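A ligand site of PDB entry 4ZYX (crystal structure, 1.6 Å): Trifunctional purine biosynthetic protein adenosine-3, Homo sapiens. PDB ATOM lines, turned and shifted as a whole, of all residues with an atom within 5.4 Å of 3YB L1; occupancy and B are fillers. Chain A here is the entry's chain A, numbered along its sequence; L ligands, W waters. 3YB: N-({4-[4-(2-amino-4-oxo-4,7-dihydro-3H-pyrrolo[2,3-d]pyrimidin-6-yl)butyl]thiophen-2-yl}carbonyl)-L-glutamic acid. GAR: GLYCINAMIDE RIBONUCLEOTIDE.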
ATOM      1  N   ASN A  37      29.965   5.908  14.490  1.00  0.00           N
ATOM      2  CA  ASN A  37      29.058   4.774  14.695  1.00  0.00           C
ATOM      3  C   ASN A  37      27.989   4.744  13.599  1.00  0.00           C
ATOM      4  O   ASN A  37      27.122   3.876  13.605  1.00  0.00           O
ATOM      5  CB  ASN A  37      28.401   4.815  16.069  1.00  0.00           C
ATOM      6  CG  ASN A  37      27.479   6.015  16.252  1.00  0.00           C
ATOM      7  OD1 ASN A  37      27.871   7.156  15.997  1.00  0.00           O
ATOM      8  ND2 ASN A  37      26.246   5.763  16.685  1.00  0.00           N
ATOM      9  N   LYS A  38      28.071   5.686  12.666  1.00  0.00           N
ATOM     10  CA  LYS A  38      27.094   5.776  11.580  1.00  0.00           C
ATOM     11  C   LYS A  38      27.763   5.950  10.222  1.00  0.00           C
ATOM     12  O   LYS A  38      28.673   6.763  10.063  1.00  0.00           O
ATOM     13  CB  LYS A  38      26.114   6.925  11.839  1.00  0.00           C
ATOM     14  CG  LYS A  38      25.168   6.665  13.002  1.00  0.00           C
ATOM     15  CD  LYS A  38      24.162   7.784  13.185  1.00  0.00           C
ATOM     16  CE  LYS A  38      23.264   7.514  14.383  1.00  0.00           C
ATOM     17  NZ  LYS A  38      22.343   8.667  14.668  1.00  0.00           N
ATOM     18  N   HIS A  59      26.962   0.478  15.822  1.00  0.00           N
ATOM     19  CA  HIS A  59      26.513  -0.035  17.119  1.00  0.00           C
ATOM     20  C   HIS A  59      25.368  -1.028  16.974  1.00  0.00           C
ATOM     21  O   HIS A  59      25.148  -1.859  17.857  1.00  0.00           O
ATOM     22  CB  HIS A  59      26.091   1.105  18.043  1.00  0.00           C
ATOM     23  CG  HIS A  59      24.883   1.852  17.573  1.00  0.00           C
ATOM     24  ND1 HIS A  59      24.943   2.875  16.662  1.00  0.00           N
ATOM     25  CD2 HIS A  59      23.566   1.707  17.896  1.00  0.00           C
ATOM     26  CE1 HIS A  59      23.715   3.341  16.435  1.00  0.00           C
ATOM     27  NE2 HIS A  59      22.871   2.635  17.170  1.00  0.00           N
ATOM     28  N   ARG A  65      26.092  -2.786  24.701  1.00  0.00           N
ATOM     29  CA  ARG A  65      26.973  -1.623  24.779  1.00  0.00           C
ATOM     30  C   ARG A  65      28.443  -2.011  24.974  1.00  0.00           C
ATOM     31  O   ARG A  65      29.341  -1.474  24.324  1.00  0.00           O
ATOM     32  CB  ARG A  65      26.504  -0.709  25.921  1.00  0.00           C
ATOM     33  CG  ARG A  65      26.673   0.782  25.651  1.00  0.00           C
ATOM     34  CD  ARG A  65      25.908   1.644  26.657  1.00  0.00           C
ATOM     35  NE  ARG A  65      24.467   1.681  26.420  1.00  0.00           N
ATOM     36  CZ  ARG A  65      23.859   2.472  25.539  1.00  0.00           C
ATOM     37  NH1 ARG A  65      24.556   3.295  24.774  1.00  0.00           N
ATOM     38  NH2 ARG A  65      22.536   2.432  25.411  1.00  0.00           N
ATOM     39  N   LEU A  86      34.884  13.098  22.050  1.00  0.00           N
ATOM     40  CA  LEU A  86      33.536  12.814  21.559  1.00  0.00           C
ATOM     41  C   LEU A  86      32.968  14.100  20.964  1.00  0.00           C
ATOM     42  O   LEU A  86      32.735  15.074  21.682  1.00  0.00           O
ATOM     43  CB  LEU A  86      32.639  12.296  22.679  1.00  0.00           C
ATOM     44  CG  LEU A  86      33.205  11.160  23.521  1.00  0.00           C
ATOM     45  CD1 LEU A  86      32.155  10.688  24.534  1.00  0.00           C
ATOM     46  CD2 LEU A  86      33.668  10.009  22.644  1.00  0.00           C
ATOM     47  N   PHE A  89      29.294  12.647  18.897  1.00  0.00           N
ATOM     48  CA  PHE A  89      29.071  11.224  19.110  1.00  0.00           C
ATOM     49  C   PHE A  89      27.906  11.051  20.075  1.00  0.00           C
ATOM     50  O   PHE A  89      27.926  11.572  21.173  1.00  0.00           O
ATOM     51  CB  PHE A  89      30.344  10.590  19.679  1.00  0.00           C
ATOM     52  CG  PHE A  89      30.263   9.106  19.877  1.00  0.00           C
ATOM     53  CD1 PHE A  89      30.395   8.249  18.803  1.00  0.00           C
ATOM     54  CD2 PHE A  89      30.083   8.578  21.147  1.00  0.00           C
ATOM     55  CE1 PHE A  89      30.343   6.873  18.989  1.00  0.00           C
ATOM     56  CE2 PHE A  89      30.033   7.198  21.350  1.00  0.00           C
ATOM     57  CZ  PHE A  89      30.159   6.357  20.274  1.00  0.00           C
ATOM     58  N   MET A  90      26.868  10.326  19.671  1.00  0.00           N
ATOM     59  CA  MET A  90      25.650  10.364  20.466  1.00  0.00           C
ATOM     60  C   MET A  90      25.342   9.088  21.271  1.00  0.00           C
ATOM     61  O   MET A  90      24.227   8.947  21.768  1.00  0.00           O
ATOM     62  CB  MET A  90      24.453  10.706  19.561  1.00  0.00           C
ATOM     63  CG  MET A  90      24.465  12.132  18.997  1.00  0.00           C
ATOM     64  SD  MET A  90      24.672  13.447  20.238  1.00  0.00           S
ATOM     65  CE  MET A  90      23.071  13.356  21.052  1.00  0.00           C
ATOM     66  N   ARG A  91      26.304   8.194  21.434  1.00  0.00           N
ATOM     67  CA  ARG A  91      26.089   6.995  22.244  1.00  0.00           C
ATOM     68  C   ARG A  91      26.590   7.140  23.674  1.00  0.00           C
ATOM     69  O   ARG A  91      27.675   7.695  23.913  1.00  0.00           O
ATOM     70  CB  ARG A  91      26.759   5.769  21.617  1.00  0.00           C
ATOM     71  CG  ARG A  91      26.417   5.518  20.159  1.00  0.00           C
ATOM     72  CD  ARG A  91      24.945   5.223  19.982  1.00  0.00           C
ATOM     73  NE  ARG A  91      24.560   3.995  20.674  1.00  0.00           N
ATOM     74  CZ  ARG A  91      23.323   3.526  20.702  1.00  0.00           C
ATOM     75  NH1 ARG A  91      22.353   4.177  20.063  1.00  0.00           N
ATOM     76  NH2 ARG A  91      23.043   2.406  21.352  1.00  0.00           N
ATOM     77  N   ILE A  92      25.806   6.640  24.615  1.00  0.00           N
ATOM     78  CA  ILE A  92      26.249   6.469  25.991  1.00  0.00           C
ATOM     79  C   ILE A  92      27.286   5.347  26.055  1.00  0.00           C
ATOM     80  O   ILE A  92      27.066   4.272  25.483  1.00  0.00           O
ATOM     81  CB  ILE A  92      25.068   6.152  26.922  1.00  0.00           C
ATOM     82  CG1 ILE A  92      24.074   7.320  26.913  1.00  0.00           C
ATOM     83  CG2 ILE A  92      25.562   5.837  28.335  1.00  0.00           C
ATOM     84  CD1 ILE A  92      22.857   7.083  27.783  1.00  0.00           C
ATOM     85  N   LEU A  93      28.407   5.590  26.722  1.00  0.00           N
ATOM     86  CA  LEU A  93      29.473   4.617  26.821  1.00  0.00           C
ATOM     87  C   LEU A  93      29.370   3.790  28.100  1.00  0.00           C
ATOM     88  O   LEU A  93      28.889   4.283  29.128  1.00  0.00           O
ATOM     89  CB  LEU A  93      30.838   5.313  26.754  1.00  0.00           C
ATOM     90  CG  LEU A  93      31.113   5.974  25.407  1.00  0.00           C
ATOM     91  CD1 LEU A  93      32.242   6.968  25.559  1.00  0.00           C
ATOM     92  CD2 LEU A  93      31.454   4.912  24.371  1.00  0.00           C
ATOM     93  N   SER A  94      29.801   2.535  28.030  1.00  0.00           N
ATOM     94  CA  SER A  94      29.757   1.632  29.178  1.00  0.00           C
ATOM     95  C   SER A  94      30.732   2.028  30.271  1.00  0.00           C
ATOM     96  O   SER A  94      31.753   2.676  30.025  1.00  0.00           O
ATOM     97  CB  SER A  94      30.050   0.200  28.736  1.00  0.00           C
ATOM     98  OG  SER A  94      31.416   0.063  28.375  1.00  0.00           O
ATOM     99  N   VAL A  98      34.591   3.792  30.012  1.00  0.00           N
ATOM    100  CA  VAL A  98      34.786   5.100  30.614  1.00  0.00           C
ATOM    101  C   VAL A  98      35.880   5.062  31.667  1.00  0.00           C
ATOM    102  O   VAL A  98      36.720   5.963  31.732  1.00  0.00           O
ATOM    103  CB  VAL A  98      33.472   5.612  31.229  1.00  0.00           C
ATOM    104  CG1 VAL A  98      33.701   6.868  32.066  1.00  0.00           C
ATOM    105  CG2 VAL A  98      32.439   5.854  30.137  1.00  0.00           C
ATOM    106  N   ASN A 107      34.283  15.360  26.128  1.00  0.00           N
ATOM    107  CA  ASN A 107      33.020  15.490  25.398  1.00  0.00           C
ATOM    108  C   ASN A 107      32.624  16.938  25.275  1.00  0.00           C
ATOM    109  O   ASN A 107      32.902  17.725  26.183  1.00  0.00           O
ATOM    110  CB  ASN A 107      31.909  14.710  26.102  1.00  0.00           C
ATOM    111  CG  ASN A 107      30.570  14.801  25.382  1.00  0.00           C
ATOM    112  OD1 ASN A 107      30.459  14.426  24.208  1.00  0.00           O
ATOM    113  ND2 ASN A 107      29.551  15.286  26.090  1.00  0.00           N
ATOM    114  N   GLY A 118      21.660  15.696  28.734  1.00  0.00           N
ATOM    115  CA  GLY A 118      20.929  14.832  27.834  1.00  0.00           C
ATOM    116  C   GLY A 118      21.131  15.135  26.369  1.00  0.00           C
ATOM    117  O   GLY A 118      21.978  15.956  26.002  1.00  0.00           O
ATOM    118  N   SER A 119      20.329  14.510  25.522  1.00  0.00           N
ATOM    119  CA  SER A 119      20.563  14.556  24.087  1.00  0.00           C
ATOM    120  C   SER A 119      19.843  15.678  23.369  1.00  0.00           C
ATOM    121  O   SER A 119      20.072  15.886  22.171  1.00  0.00           O
ATOM    122  CB  SER A 119      20.176  13.219  23.453  1.00  0.00           C
ATOM    123  OG  SER A 119      18.774  13.038  23.583  1.00  0.00           O
ATOM    124  N   HIS A 138      33.859  18.682  28.906  1.00  0.00           N
ATOM    125  CA  HIS A 138      34.079  18.022  30.187  1.00  0.00           C
ATOM    126  C   HIS A 138      34.761  16.679  29.996  1.00  0.00           C
ATOM    127  O   HIS A 138      34.658  16.054  28.944  1.00  0.00           O
ATOM    128  CB  HIS A 138      32.755  17.833  30.935  1.00  0.00           C
ATOM    129  CG  HIS A 138      31.779  16.960  30.221  1.00  0.00           C
ATOM    130  ND1 HIS A 138      31.655  15.615  30.492  1.00  0.00           N
ATOM    131  CD2 HIS A 138      30.879  17.230  29.250  1.00  0.00           C
ATOM    132  CE1 HIS A 138      30.724  15.097  29.706  1.00  0.00           C
ATOM    133  NE2 HIS A 138      30.238  16.052  28.939  1.00  0.00           N
ATOM    134  N   VAL A 140      34.783  12.829  30.451  1.00  0.00           N
ATOM    135  CA  VAL A 140      33.688  11.862  30.470  1.00  0.00           C
ATOM    136  C   VAL A 140      33.757  10.957  31.692  1.00  0.00           C
ATOM    137  O   VAL A 140      34.764  10.250  31.902  1.00  0.00           O
ATOM    138  CB  VAL A 140      33.697  11.034  29.180  1.00  0.00           C
ATOM    139  CG1 VAL A 140      32.679   9.897  29.264  1.00  0.00           C
ATOM    140  CG2 VAL A 140      33.396  11.938  27.996  1.00  0.00           C
ATOM    141  N   ALA A 141      32.698  10.993  32.496  1.00  0.00           N
ATOM    142  CA  ALA A 141      32.549  10.108  33.652  1.00  0.00           C
ATOM    143  C   ALA A 141      31.423   9.127  33.372  1.00  0.00           C
ATOM    144  O   ALA A 141      30.717   9.275  32.383  1.00  0.00           O
ATOM    145  CB  ALA A 141      32.268  10.898  34.920  1.00  0.00           C
ATOM    146  N   GLU A 142      31.236   8.120  34.221  1.00  0.00           N
ATOM    147  CA  GLU A 142      30.212   7.126  33.916  1.00  0.00           C
ATOM    148  C   GLU A 142      28.827   7.755  33.880  1.00  0.00           C
ATOM    149  O   GLU A 142      28.038   7.469  32.989  1.00  0.00           O
ATOM    150  CB  GLU A 142      30.259   5.971  34.923  1.00  0.00           C
ATOM    151  CG  GLU A 142      29.246   4.885  34.590  1.00  0.00           C
ATOM    152  CD  GLU A 142      29.536   3.560  35.266  1.00  0.00           C
ATOM    153  OE1 GLU A 142      30.516   3.484  36.027  1.00  0.00           O
ATOM    154  OE2 GLU A 142      28.776   2.604  35.019  1.00  0.00           O
ATOM    155  N   ASP A 143      28.529   8.617  34.851  1.00  0.00           N
ATOM    156  CA  ASP A 143      27.258   9.346  34.835  1.00  0.00           C
ATOM    157  C   ASP A 143      27.289  10.390  33.729  1.00  0.00           C
ATOM    158  O   ASP A 143      28.144  11.270  33.709  1.00  0.00           O
ATOM    159  CB  ASP A 143      26.975   9.994  36.176  1.00  0.00           C
ATOM    160  CG  ASP A 143      26.555   8.989  37.219  1.00  0.00           C
ATOM    161  OD1 ASP A 143      25.854   8.018  36.857  1.00  0.00           O
ATOM    162  OD2 ASP A 143      26.917   9.165  38.400  1.00  0.00           O
ATOM    163  N   VAL A 144      26.332  10.275  32.811  1.00  0.00           N
ATOM    164  CA  VAL A 144      26.325  11.092  31.598  1.00  0.00           C
ATOM    165  C   VAL A 144      26.227  12.591  31.873  1.00  0.00           C
ATOM    166  O   VAL A 144      25.398  13.048  32.671  1.00  0.00           O
ATOM    167  CB  VAL A 144      25.166  10.664  30.675  1.00  0.00           C
ATOM    168  CG1 VAL A 144      25.110  11.534  29.431  1.00  0.00           C
ATOM    169  CG2 VAL A 144      25.341   9.206  30.284  1.00  0.00           C
ATOM    170  N   ASP A 145      27.114  13.345  31.217  1.00  0.00           N
ATOM    171  CA  ASP A 145      27.186  14.808  31.308  1.00  0.00           C
ATOM    172  C   ASP A 145      27.439  15.306  32.726  1.00  0.00           C
ATOM    173  O   ASP A 145      27.081  16.441  33.071  1.00  0.00           O
ATOM    174  CB  ASP A 145      25.892  15.436  30.750  1.00  0.00           C
ATOM    175  CG  ASP A 145      25.684  15.128  29.273  1.00  0.00           C
ATOM    176  OD1 ASP A 145      26.676  14.801  28.576  1.00  0.00           O
ATOM    177  OD2 ASP A 145      24.541  15.214  28.796  1.00  0.00           O
ATOM    178  N   ALA A 146      28.095  14.484  33.541  1.00  0.00           N
ATOM    179  CA  ALA A 146      28.372  14.834  34.940  1.00  0.00           C
ATOM    180  C   ALA A 146      29.859  14.878  35.269  1.00  0.00           C
ATOM    181  O   ALA A 146      30.230  15.196  36.407  1.00  0.00           O
ATOM    182  CB  ALA A 146      27.661  13.863  35.884  1.00  0.00           C
HETATM  183  N1  3YB L   1      28.808   8.239  28.101  1.00  0.00           N
HETATM  184  C2  3YB L   1      29.016   8.341  29.414  1.00  0.00           C
HETATM  185  N3  3YB L   1      29.203   9.546  29.992  1.00  0.00           N
HETATM  186  C4  3YB L   1      29.175  10.690  29.272  1.00  0.00           C
HETATM  187  N5  3YB L   1      28.590   9.456  26.026  1.00  0.00           N
HETATM  188  C6  3YB L   1      28.617  10.758  25.669  1.00  0.00           C
HETATM  189  C7  3YB L   1      28.876  11.510  26.809  1.00  0.00           C
HETATM  190  C8  3YB L   1      28.966  10.611  27.887  1.00  0.00           C
HETATM  191  C9  3YB L   1      28.779   9.342  27.335  1.00  0.00           C
HETATM  192  O10 3YB L   1      29.352  11.758  29.877  1.00  0.00           O
HETATM  193  N11 3YB L   1      29.051   7.178  30.241  1.00  0.00           N
HETATM  194  C12 3YB L   1      23.177  10.547  24.435  1.00  0.00           C
HETATM  195  C13 3YB L   1      22.104   9.955  25.027  1.00  0.00           C
HETATM  196  S14 3YB L   1      21.805  10.898  26.417  1.00  0.00           S
HETATM  197  C15 3YB L   1      23.059  12.049  26.233  1.00  0.00           C
HETATM  198  C16 3YB L   1      23.698  11.701  25.084  1.00  0.00           C
HETATM  199  C17 3YB L   1      21.399   8.767  24.588  1.00  0.00           C
HETATM  200  O18 3YB L   1      20.360   8.475  25.161  1.00  0.00           O
HETATM  201  N19 3YB L   1      21.919   7.958  23.521  1.00  0.00           N
HETATM  202  C20 3YB L   1      21.286   6.841  23.099  1.00  0.00           C
HETATM  203  C21 3YB L   1      21.213   6.802  21.682  1.00  0.00           C
HETATM  204  C22 3YB L   1      21.099   8.162  21.095  1.00  0.00           C
HETATM  205  C23 3YB L   1      21.201   8.076  19.609  1.00  0.00           C
HETATM  206  O24 3YB L   1      21.861   7.126  19.074  1.00  0.00           O
HETATM  207  O25 3YB L   1      20.634   8.939  18.892  1.00  0.00           O
HETATM  208  C26 3YB L   1      21.982   5.682  23.512  1.00  0.00           C
HETATM  209  O27 3YB L   1      21.339   4.609  23.680  1.00  0.00           O
HETATM  210  O28 3YB L   1      23.228   5.687  23.698  1.00  0.00           O
HETATM  211  C29 3YB L   1      28.455  11.256  24.272  1.00  0.00           C
HETATM  212  C30 3YB L   1      27.286  12.203  24.217  1.00  0.00           C
HETATM  213  C31 3YB L   1      26.043  11.499  24.599  1.00  0.00           C
HETATM  214  C32 3YB L   1      24.880  12.429  24.546  1.00  0.00           C
HETATM  215  C1  GAR L   2      27.149  19.604  18.688  1.00  0.00           C
HETATM  216  O6  GAR L   2      26.339  20.762  18.858  1.00  0.00           O
HETATM  217  C2  GAR L   2      27.374  18.931  20.019  1.00  0.00           C
HETATM  218  O8  GAR L   2      27.578  19.838  21.113  1.00  0.00           O
HETATM  219  C3  GAR L   2      26.084  18.130  20.191  1.00  0.00           C
HETATM  220  O4  GAR L   2      25.875  17.614  18.878  1.00  0.00           O
HETATM  221  C5  GAR L   2      26.344  18.571  17.914  1.00  0.00           C
HETATM  222  C10 GAR L   2      27.242  17.880  16.915  1.00  0.00           C
HETATM  223  O12 GAR L   2      27.534  18.763  15.842  1.00  0.00           O
HETATM  224  N19 GAR L   2      26.217  17.093  21.196  1.00  0.00           N
HETATM  225  C21 GAR L   2      25.197  16.810  22.002  1.00  0.00           C
HETATM  226  O22 GAR L   2      24.079  17.282  21.880  1.00  0.00           O
HETATM  227  C23 GAR L   2      25.463  15.818  23.114  1.00  0.00           C
HETATM  228  N24 GAR L   2      26.872  15.579  23.291  1.00  0.00           N
HETATM  229  P15 GAR L   2      28.742  18.423  14.825  1.00  0.00           P
HETATM  230  O16 GAR L   2      28.583  19.494  13.759  1.00  0.00           O
HETATM  231  O17 GAR L   2      28.474  17.002  14.356  1.00  0.00           O
HETATM  232  O18 GAR L   2      29.969  18.517  15.667  1.00  0.00           O
HETATM  233  O   HOH W   1      24.218   7.769  17.465  1.00  0.00           O
HETATM  234  O   HOH W   2      30.235  12.503  32.328  1.00  0.00           O
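O of Ile 92 lies within hydrogen-bond range of NH1 of Arg 65 (2.8 Å).
A ring nitrogen (NE2) of His 59 is in hydrogen-bond range of the guanidinium group of Arg 91 (3.3 Å).
The backbone NH (N) of Gly 118 sits at hydrogen-bond distance from the side-chain carboxylate (OD2) of Asp 145, at 2.9 Å.
The backbone NH (N) of Asn 107 is in hydrogen-bond range of the backbone carbonyl oxygen (O) of His 138, at 2.9 Å.
The backbone carbonyl oxygen (O) of Leu 86 sits close to the side-chain amide oxygen (OD1) of Asn 107.
Water W1 lies within hydrogen-bond range of O24 of 3YB L1, ND2 of Asn 37 and NZ of Lys 38.
Merely in contact with 3YB L1: Phe 89 (3.2 Å), Val 144 (3.5 Å), Val 140 (3.6 Å), His 138 (3.6 Å), Val 98 (3.6 Å), Gly 118 (3.6 Å), Leu 86 (3.7 Å), Ser 119 (3.7 Å) and Asn 107 (3.8 Å).
Within 4 Å of 3YB L1: Arg 65, Leu 86, Phe 89, Met 90, Arg 91, Ile 92, Leu 93, Val 98, Asn 107, Gly 118, Ser 119, His 138, Val 140, Ala 141, Glu 142, Val 144 and Asp 145.
The backbone carbonyl oxygen (O) of Ala 141 lies within hydrogen-bond range of a nitrogen (N3) of 3YB L1 (2.8 Å).
The backbone NH of Ile 92 lies within hydrogen-bond range of an oxygen (O28) of 3YB L1 (2.9 Å).
O of Arg 91 sits at hydrogen-bond distance from N5 of 3YB L1 (2.9 Å).
An oxygen (O24) of 3YB L1 is in salt-bridge range of the guanidinium group (NH1) of Arg 91 (3.1 Å).
An oxygen (O28) of 3YB L1 is in salt-bridge range of the guanidinium group (NH1) of Arg 65.
The backbone carbonyl oxygen of Glu 142 lies within hydrogen-bond range of a nitrogen (N11) of 3YB L1 (2.9 Å).
N1 of 3YB L1 lies within hydrogen-bond range of N of Leu 93.
O of Leu 93 lies within hydrogen-bond range of N11 of 3YB L1 (3.1 Å).
The backbone NH (N) of Asp 145 sits at hydrogen-bond distance from an oxygen (O10) of 3YB L1, at 3.1 Å.
A nitrogen (N19) of 3YB L1 sits at hydrogen-bond distance from the backbone carbonyl oxygen of Met 90 (3.1 Å).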
